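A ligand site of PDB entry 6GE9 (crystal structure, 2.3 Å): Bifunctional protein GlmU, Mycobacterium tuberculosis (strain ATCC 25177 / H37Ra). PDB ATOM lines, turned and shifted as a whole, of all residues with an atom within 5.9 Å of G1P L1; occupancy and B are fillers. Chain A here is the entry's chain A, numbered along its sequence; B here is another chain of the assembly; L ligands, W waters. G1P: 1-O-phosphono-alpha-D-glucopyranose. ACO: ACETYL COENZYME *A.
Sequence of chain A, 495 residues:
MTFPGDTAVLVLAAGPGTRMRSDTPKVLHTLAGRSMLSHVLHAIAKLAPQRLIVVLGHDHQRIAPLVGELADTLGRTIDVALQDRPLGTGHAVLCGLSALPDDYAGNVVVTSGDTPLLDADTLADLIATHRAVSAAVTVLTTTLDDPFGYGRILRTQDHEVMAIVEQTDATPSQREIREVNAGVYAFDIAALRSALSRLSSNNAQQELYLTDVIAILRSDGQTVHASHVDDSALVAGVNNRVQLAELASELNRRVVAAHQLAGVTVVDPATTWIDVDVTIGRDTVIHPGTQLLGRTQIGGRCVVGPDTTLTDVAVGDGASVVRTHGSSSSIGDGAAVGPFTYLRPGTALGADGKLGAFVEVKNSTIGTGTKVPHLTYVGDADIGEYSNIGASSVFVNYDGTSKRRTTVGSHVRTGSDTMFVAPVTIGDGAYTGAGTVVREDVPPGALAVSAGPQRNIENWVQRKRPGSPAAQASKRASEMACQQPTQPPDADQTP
Pro 373 of chain B touches G1P L1 (CG to O3, 3.5 Å).
Hydrophobic or aromatic side chains within 4 Å of G1P L1: Tyr 377, Pro 373 of chain B and His 374 of chain B.
Of the 17 residues printed, 8 come within 4 Å of G1P L1.
Along chain A the residues within 4 Å of G1P L1 span positions 344 to 403.
The nearest printed residue that does not touch G1P L1 is Tyr 398 (4.01 Å).
O of ACO L2 lies within hydrogen-bond range of O3 of G1P L1.
The guanidinium group (NH1) of Arg 344 is in salt-bridge range of the side-chain carboxylate (OE2) of Glu 360.
ND1 of His 374 of chain B is in hydrogen-bond range of OE1 of Glu 360 (2.6 Å).
O of Tyr 377 lies within hydrogen-bond range of N of Phe 395 (3.0 Å).
The side-chain amino group (NZ) of Lys 362 lies within salt-bridge range of the side-chain carboxylate (OD2) of Asp 380 (3.2 Å).
The side-chain amide nitrogen (ND2) of Asn 397 sits at hydrogen-bond distance from the side-chain carboxylate (OD2) of Asp 380, at 2.7 Å.
An oxygen (O4) of G1P L1 sits at hydrogen-bond distance from the side-chain amide oxygen (OD1) of Asn 388 of chain B.
The side-chain amino group (NZ) of Lys 403 lies within salt-bridge range of an oxygen (O1P) of G1P L1 (3.4 Å).
The guanidinium group (NH2) of Arg 344 lies within salt-bridge range of an oxygen (O2P) of G1P L1.
The backbone carbonyl oxygen (O) of Tyr 398 sits at hydrogen-bond distance from a nitrogen (N4P) of ACO L2.
The side-chain hydroxyl (OH) of Tyr 377 is in hydrogen-bond range of an oxygen (O2P) of G1P L1, at 2.9 Å.
The side-chain amide nitrogen of Asn 397 sits at hydrogen-bond distance from an oxygen (O1P) of G1P L1 (3.2 Å).
An oxygen (O2) of G1P L1 lies within hydrogen-bond range of a ring nitrogen (NE2) of His 374 of chain B.
The side-chain amino group (NZ) of Lys 362 lies within salt-bridge range of an oxygen (O1P) of G1P L1, 2.7 Å away.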
ATOM      1  N   ARG A 344      10.453  22.186  35.554  1.00  0.00           N
ATOM      2  CA  ARG A 344      11.487  23.202  35.490  1.00  0.00           C
ATOM      3  C   ARG A 344      10.973  24.419  34.737  1.00  0.00           C
ATOM      4  O   ARG A 344       9.953  24.350  34.049  1.00  0.00           O
ATOM      5  CB  ARG A 344      12.724  22.634  34.789  1.00  0.00           C
ATOM      6  CG  ARG A 344      13.246  21.352  35.411  1.00  0.00           C
ATOM      7  CD  ARG A 344      14.507  21.598  36.214  1.00  0.00           C
ATOM      8  NE  ARG A 344      15.583  22.171  35.400  1.00  0.00           N
ATOM      9  CZ  ARG A 344      16.339  21.471  34.564  1.00  0.00           C
ATOM     10  NH1 ARG A 344      16.150  20.163  34.424  1.00  0.00           N
ATOM     11  NH2 ARG A 344      17.297  22.073  33.879  1.00  0.00           N
ATOM     12  N   GLU A 360      10.143  14.536  34.307  1.00  0.00           N
ATOM     13  CA  GLU A 360      10.777  15.841  34.447  1.00  0.00           C
ATOM     14  C   GLU A 360      10.708  16.589  33.120  1.00  0.00           C
ATOM     15  O   GLU A 360      11.096  16.031  32.081  1.00  0.00           O
ATOM     16  CB  GLU A 360      12.234  15.714  34.907  1.00  0.00           C
ATOM     17  CG  GLU A 360      12.976  17.041  34.946  1.00  0.00           C
ATOM     18  CD  GLU A 360      14.446  16.881  35.271  1.00  0.00           C
ATOM     19  OE1 GLU A 360      14.885  15.735  35.509  1.00  0.00           O
ATOM     20  OE2 GLU A 360      15.169  17.896  35.293  1.00  0.00           O
ATOM     21  N   LYS A 362      11.637  20.372  31.198  1.00  0.00           N
ATOM     22  CA  LYS A 362      12.455  21.577  31.289  1.00  0.00           C
ATOM     23  C   LYS A 362      12.430  22.292  29.952  1.00  0.00           C
ATOM     24  O   LYS A 362      12.895  21.754  28.947  1.00  0.00           O
ATOM     25  CB  LYS A 362      13.894  21.232  31.681  1.00  0.00           C
ATOM     26  CG  LYS A 362      14.863  22.399  31.552  1.00  0.00           C
ATOM     27  CD  LYS A 362      15.863  22.173  30.432  1.00  0.00           C
ATOM     28  CE  LYS A 362      16.914  23.274  30.402  1.00  0.00           C
ATOM     29  NZ  LYS A 362      17.952  23.009  29.369  1.00  0.00           N
ATOM     30  N   TYR A 377      12.113  12.096  30.685  1.00  0.00           N
ATOM     31  CA  TYR A 377      12.695  13.428  30.749  1.00  0.00           C
ATOM     32  C   TYR A 377      12.421  14.142  29.427  1.00  0.00           C
ATOM     33  O   TYR A 377      12.755  13.627  28.364  1.00  0.00           O
ATOM     34  CB  TYR A 377      14.196  13.384  31.035  1.00  0.00           C
ATOM     35  CG  TYR A 377      14.885  14.708  30.794  1.00  0.00           C
ATOM     36  CD1 TYR A 377      14.784  15.736  31.728  1.00  0.00           C
ATOM     37  CD2 TYR A 377      15.623  14.936  29.646  1.00  0.00           C
ATOM     38  CE1 TYR A 377      15.410  16.952  31.521  1.00  0.00           C
ATOM     39  CE2 TYR A 377      16.242  16.155  29.434  1.00  0.00           C
ATOM     40  CZ  TYR A 377      16.135  17.151  30.372  1.00  0.00           C
ATOM     41  OH  TYR A 377      16.761  18.366  30.165  1.00  0.00           O
ATOM     42  N   GLY A 379      13.306  17.643  27.768  1.00  0.00           N
ATOM     43  CA  GLY A 379      14.071  18.879  27.843  1.00  0.00           C
ATOM     44  C   GLY A 379      14.280  19.535  26.506  1.00  0.00           C
ATOM     45  O   GLY A 379      14.737  18.894  25.556  1.00  0.00           O
ATOM     46  N   ASP A 380      13.954  20.831  26.416  1.00  0.00           N
ATOM     47  CA  ASP A 380      14.134  21.626  25.196  1.00  0.00           C
ATOM     48  C   ASP A 380      13.434  20.970  24.009  1.00  0.00           C
ATOM     49  O   ASP A 380      14.039  20.708  22.958  1.00  0.00           O
ATOM     50  CB  ASP A 380      15.611  21.862  24.906  1.00  0.00           C
ATOM     51  CG  ASP A 380      16.326  22.537  26.065  1.00  0.00           C
ATOM     52  OD1 ASP A 380      15.713  23.383  26.744  1.00  0.00           O
ATOM     53  OD2 ASP A 380      17.517  22.228  26.292  1.00  0.00           O
ATOM     54  N   PHE A 395      14.426  12.827  25.981  1.00  0.00           N
ATOM     55  CA  PHE A 395      14.694  13.806  24.929  1.00  0.00           C
ATOM     56  C   PHE A 395      16.130  14.281  25.101  1.00  0.00           C
ATOM     57  O   PHE A 395      16.414  15.192  25.876  1.00  0.00           O
ATOM     58  CB  PHE A 395      13.696  14.955  24.999  1.00  0.00           C
ATOM     59  CG  PHE A 395      12.337  14.610  24.454  1.00  0.00           C
ATOM     60  CD1 PHE A 395      11.453  13.838  25.196  1.00  0.00           C
ATOM     61  CD2 PHE A 395      11.945  15.054  23.209  1.00  0.00           C
ATOM     62  CE1 PHE A 395      10.201  13.522  24.706  1.00  0.00           C
ATOM     63  CE2 PHE A 395      10.688  14.738  22.706  1.00  0.00           C
ATOM     64  CZ  PHE A 395       9.825  13.966  23.455  1.00  0.00           C
ATOM     65  N   ASN A 397      19.035  16.274  24.806  1.00  0.00           N
ATOM     66  CA  ASN A 397      19.257  17.661  24.412  1.00  0.00           C
ATOM     67  C   ASN A 397      20.666  18.140  24.755  1.00  0.00           C
ATOM     68  O   ASN A 397      20.888  19.343  24.907  1.00  0.00           O
ATOM     69  CB  ASN A 397      18.225  18.576  25.079  1.00  0.00           C
ATOM     70  CG  ASN A 397      18.387  18.643  26.587  1.00  0.00           C
ATOM     71  OD1 ASN A 397      18.844  17.680  27.221  1.00  0.00           O
ATOM     72  ND2 ASN A 397      18.022  19.768  27.179  1.00  0.00           N
ATOM     73  N   TYR A 398      21.631  17.224  24.871  1.00  0.00           N
ATOM     74  CA  TYR A 398      22.991  17.598  25.250  1.00  0.00           C
ATOM     75  C   TYR A 398      23.952  16.603  24.611  1.00  0.00           C
ATOM     76  O   TYR A 398      24.026  15.446  25.040  1.00  0.00           O
ATOM     77  CB  TYR A 398      23.150  17.621  26.770  1.00  0.00           C
ATOM     78  CG  TYR A 398      24.513  18.079  27.239  1.00  0.00           C
ATOM     79  CD1 TYR A 398      25.014  19.324  26.875  1.00  0.00           C
ATOM     80  CD2 TYR A 398      25.296  17.266  28.053  1.00  0.00           C
ATOM     81  CE1 TYR A 398      26.259  19.742  27.315  1.00  0.00           C
ATOM     82  CE2 TYR A 398      26.536  17.676  28.495  1.00  0.00           C
ATOM     83  CZ  TYR A 398      27.020  18.916  28.115  1.00  0.00           C
ATOM     84  OH  TYR A 398      28.252  19.329  28.552  1.00  0.00           O
ATOM     85  N   LYS A 403      23.437  22.478  23.529  1.00  0.00           N
ATOM     86  CA  LYS A 403      22.069  21.997  23.685  1.00  0.00           C
ATOM     87  C   LYS A 403      21.311  22.139  22.378  1.00  0.00           C
ATOM     88  O   LYS A 403      21.405  23.178  21.706  1.00  0.00           O
ATOM     89  CB  LYS A 403      21.350  22.749  24.802  1.00  0.00           C
ATOM     90  CG  LYS A 403      22.165  22.917  26.070  1.00  0.00           C
ATOM     91  CD  LYS A 403      21.941  21.760  27.032  1.00  0.00           C
ATOM     92  CE  LYS A 403      21.228  22.228  28.301  1.00  0.00           C
ATOM     93  NZ  LYS A 403      22.055  22.015  29.518  1.00  0.00           N
ATOM     94  N   LYS B 371      27.878  14.905  37.471  1.00  0.00           N
ATOM     95  CA  LYS B 371      26.437  15.125  37.480  1.00  0.00           C
ATOM     96  C   LYS B 371      25.716  13.868  37.031  1.00  0.00           C
ATOM     97  O   LYS B 371      26.057  13.294  35.992  1.00  0.00           O
ATOM     98  CB  LYS B 371      26.057  16.313  36.593  1.00  0.00           C
ATOM     99  CG  LYS B 371      26.717  17.624  36.998  1.00  0.00           C
ATOM    100  CD  LYS B 371      26.300  18.751  36.067  1.00  0.00           C
ATOM    101  CE  LYS B 371      26.886  20.077  36.530  1.00  0.00           C
ATOM    102  NZ  LYS B 371      26.443  21.206  35.673  1.00  0.00           N
ATOM    103  N   PRO B 373      21.900  13.534  36.393  1.00  0.00           N
ATOM    104  CA  PRO B 373      20.731  14.409  36.483  1.00  0.00           C
ATOM    105  C   PRO B 373      19.370  13.727  36.510  1.00  0.00           C
ATOM    106  O   PRO B 373      18.492  14.166  37.268  1.00  0.00           O
ATOM    107  CB  PRO B 373      20.872  15.295  35.231  1.00  0.00           C
ATOM    108  CG  PRO B 373      22.259  15.044  34.699  1.00  0.00           C
ATOM    109  CD  PRO B 373      22.572  13.641  35.089  1.00  0.00           C
ATOM    110  N   HIS B 374      19.134  12.700  35.699  1.00  0.00           N
ATOM    111  CA  HIS B 374      17.770  12.213  35.528  1.00  0.00           C
ATOM    112  C   HIS B 374      17.703  10.692  35.500  1.00  0.00           C
ATOM    113  O   HIS B 374      18.511  10.029  34.839  1.00  0.00           O
ATOM    114  CB  HIS B 374      17.137  12.745  34.238  1.00  0.00           C
ATOM    115  CG  HIS B 374      17.630  14.093  33.824  1.00  0.00           C
ATOM    116  ND1 HIS B 374      17.221  15.256  34.450  1.00  0.00           N
ATOM    117  CD2 HIS B 374      18.480  14.477  32.847  1.00  0.00           C
ATOM    118  CE1 HIS B 374      17.812  16.295  33.873  1.00  0.00           C
ATOM    119  NE2 HIS B 374      18.577  15.848  32.899  1.00  0.00           N
ATOM    120  N   ASN B 388      29.578  13.163  33.384  1.00  0.00           N
ATOM    121  CA  ASN B 388      28.146  13.394  33.183  1.00  0.00           C
ATOM    122  C   ASN B 388      27.506  12.097  32.742  1.00  0.00           C
ATOM    123  O   ASN B 388      27.862  11.547  31.697  1.00  0.00           O
ATOM    124  CB  ASN B 388      27.905  14.500  32.156  1.00  0.00           C
ATOM    125  CG  ASN B 388      26.468  14.980  32.132  1.00  0.00           C
ATOM    126  OD1 ASN B 388      26.094  15.882  32.883  1.00  0.00           O
ATOM    127  ND2 ASN B 388      25.656  14.378  31.271  1.00  0.00           N
ATOM    128  N   ILE B 389      26.570  11.598  33.539  1.00  0.00           N
ATOM    129  CA  ILE B 389      25.865  10.353  33.261  1.00  0.00           C
ATOM    130  C   ILE B 389      24.525  10.697  32.617  1.00  0.00           C
ATOM    131  O   ILE B 389      23.722  11.432  33.191  1.00  0.00           O
ATOM    132  CB  ILE B 389      25.668   9.508  34.526  1.00  0.00           C
ATOM    133  CG1 ILE B 389      27.014   9.286  35.226  1.00  0.00           C
ATOM    134  CG2 ILE B 389      25.001   8.186  34.198  1.00  0.00           C
ATOM    135  CD1 ILE B 389      28.040   8.571  34.369  1.00  0.00           C
ATOM    136  N   GLY B 390      24.281  10.151  31.419  1.00  0.00           N
ATOM    137  CA  GLY B 390      23.046  10.424  30.727  1.00  0.00           C
ATOM    138  C   GLY B 390      21.840   9.882  31.468  1.00  0.00           C
ATOM    139  O   GLY B 390      21.938   9.030  32.349  1.00  0.00           O
ATOM    140  N   ALA B 391      20.673  10.406  31.093  1.00  0.00           N
ATOM    141  CA  ALA B 391      19.425  10.011  31.732  1.00  0.00           C
ATOM    142  C   ALA B 391      19.071   8.573  31.385  1.00  0.00           C
ATOM    143  O   ALA B 391      19.594   7.985  30.433  1.00  0.00           O
ATOM    144  CB  ALA B 391      18.291  10.946  31.310  1.00  0.00           C
HETATM  145  C1  G1P L   1      20.973  18.748  30.369  1.00  0.00           C
HETATM  146  C2  G1P L   1      21.250  17.251  30.281  1.00  0.00           C
HETATM  147  C3  G1P L   1      22.110  16.807  31.460  1.00  0.00           C
HETATM  148  C4  G1P L   1      23.349  17.675  31.582  1.00  0.00           C
HETATM  149  C5  G1P L   1      22.983  19.149  31.595  1.00  0.00           C
HETATM  150  C6  G1P L   1      24.234  20.025  31.595  1.00  0.00           C
HETATM  151  O1  G1P L   1      20.168  19.010  31.517  1.00  0.00           O
HETATM  152  O2  G1P L   1      20.008  16.537  30.304  1.00  0.00           O
HETATM  153  O3  G1P L   1      22.504  15.440  31.276  1.00  0.00           O
HETATM  154  O4  G1P L   1      24.046  17.350  32.795  1.00  0.00           O
HETATM  155  O5  G1P L   1      22.206  19.468  30.437  1.00  0.00           O
HETATM  156  O6  G1P L   1      23.853  21.386  31.383  1.00  0.00           O
HETATM  157  P   G1P L   1      19.240  20.312  31.593  1.00  0.00           P
HETATM  158  O1P G1P L   1      18.981  20.662  30.151  1.00  0.00           O
HETATM  159  O2P G1P L   1      18.022  19.857  32.353  1.00  0.00           O
HETATM  160  O3P G1P L   1      20.090  21.323  32.324  1.00  0.00           O
HETATM  161  N1A ACO L   2      23.605   4.480  18.889  1.00  0.00           N
HETATM  162  C2A ACO L   2      24.231   3.593  18.091  1.00  0.00           C
HETATM  163  N3A ACO L   2      25.200   3.929  17.229  1.00  0.00           N
HETATM  164  C4A ACO L   2      25.608   5.213  17.097  1.00  0.00           C
HETATM  165  C5A ACO L   2      24.964   6.245  17.928  1.00  0.00           C
HETATM  166  C6A ACO L   2      23.901   5.795  18.863  1.00  0.00           C
HETATM  167  N6A ACO L   2      23.259   6.682  19.666  1.00  0.00           N
HETATM  168  N7A ACO L   2      25.547   7.412  17.619  1.00  0.00           N
HETATM  169  C8A ACO L   2      26.481   7.152  16.661  1.00  0.00           C
HETATM  170  N9A ACO L   2      26.507   5.850  16.353  1.00  0.00           N
HETATM  171  C1B ACO L   2      27.416   5.215  15.363  1.00  0.00           C
HETATM  172  C2B ACO L   2      27.184   5.769  13.966  1.00  0.00           C
HETATM  173  O2B ACO L   2      26.461   4.848  13.152  1.00  0.00           O
HETATM  174  C3B ACO L   2      28.577   5.991  13.414  1.00  0.00           C
HETATM  175  O3B ACO L   2      29.028   4.806  12.770  1.00  0.00           O
HETATM  176  P3B ACO L   2      29.324   4.730  11.185  1.00  0.00           P
HETATM  177  O7A ACO L   2      29.169   6.153  10.716  1.00  0.00           O
HETATM  178  O8A ACO L   2      28.284   3.768  10.662  1.00  0.00           O
HETATM  179  O9A ACO L   2      30.741   4.215  11.122  1.00  0.00           O
HETATM  180  C4B ACO L   2      29.441   6.176  14.644  1.00  0.00           C
HETATM  181  O4B ACO L   2      28.758   5.560  15.728  1.00  0.00           O
HETATM  182  C5B ACO L   2      29.652   7.651  14.994  1.00  0.00           C
HETATM  183  O5B ACO L   2      29.958   8.414  13.835  1.00  0.00           O
HETATM  184  P1A ACO L   2      29.438   9.930  13.758  1.00  0.00           P
HETATM  185  O1A ACO L   2      28.162   9.953  12.955  1.00  0.00           O
HETATM  186  O2A ACO L   2      30.602  10.814  13.346  1.00  0.00           O
HETATM  187  O3A ACO L   2      29.089  10.240  15.298  1.00  0.00           O
HETATM  188  P2A ACO L   2      28.276  11.569  15.715  1.00  0.00           P
HETATM  189  O4A ACO L   2      29.242  12.737  15.720  1.00  0.00           O
HETATM  190  O5A ACO L   2      26.999  11.642  14.909  1.00  0.00           O
HETATM  191  O6A ACO L   2      27.879  11.239  17.241  1.00  0.00           O
HETATM  192  CBP ACO L   2      26.410  11.068  19.144  1.00  0.00           C
HETATM  193  CCP ACO L   2      26.581  11.579  17.725  1.00  0.00           C
HETATM  194  CDP ACO L   2      26.955  12.112  20.105  1.00  0.00           C
HETATM  195  CEP ACO L   2      27.171   9.761  19.318  1.00  0.00           C
HETATM  196  CAP ACO L   2      24.914  10.839  19.372  1.00  0.00           C
HETATM  197  OAP ACO L   2      24.438   9.893  18.398  1.00  0.00           O
HETATM  198  C9P ACO L   2      24.603  10.324  20.745  1.00  0.00           C
HETATM  199  O9P ACO L   2      24.542   9.127  20.966  1.00  0.00           O
HETATM  200  N8P ACO L   2      24.380  11.236  21.679  1.00  0.00           N
HETATM  201  C7P ACO L   2      23.932  10.901  23.014  1.00  0.00           C
HETATM  202  C6P ACO L   2      24.297  12.010  23.995  1.00  0.00           C
HETATM  203  C5P ACO L   2      23.558  11.813  25.296  1.00  0.00           C
HETATM  204  O5P ACO L   2      22.718  10.936  25.403  1.00  0.00           O
HETATM  205  N4P ACO L   2      23.860  12.656  26.278  1.00  0.00           N
HETATM  206  C3P ACO L   2      23.735  12.278  27.667  1.00  0.00           C
HETATM  207  C2P ACO L   2      23.040  13.354  28.487  1.00  0.00           C
HETATM  208  S1P ACO L   2      21.694  13.993  27.551  1.00  0.00           S
HETATM  209  C   ACO L   2      20.494  13.953  28.698  1.00  0.00           C
HETATM  210  O   ACO L   2      20.784  13.691  29.858  1.00  0.00           O
HETATM  211  CH3 ACO L   2      19.075  14.214  28.277  1.00  0.00           C
HETATM  212  O   HOH W   1      21.829  18.671  34.965  1.00  0.00           O
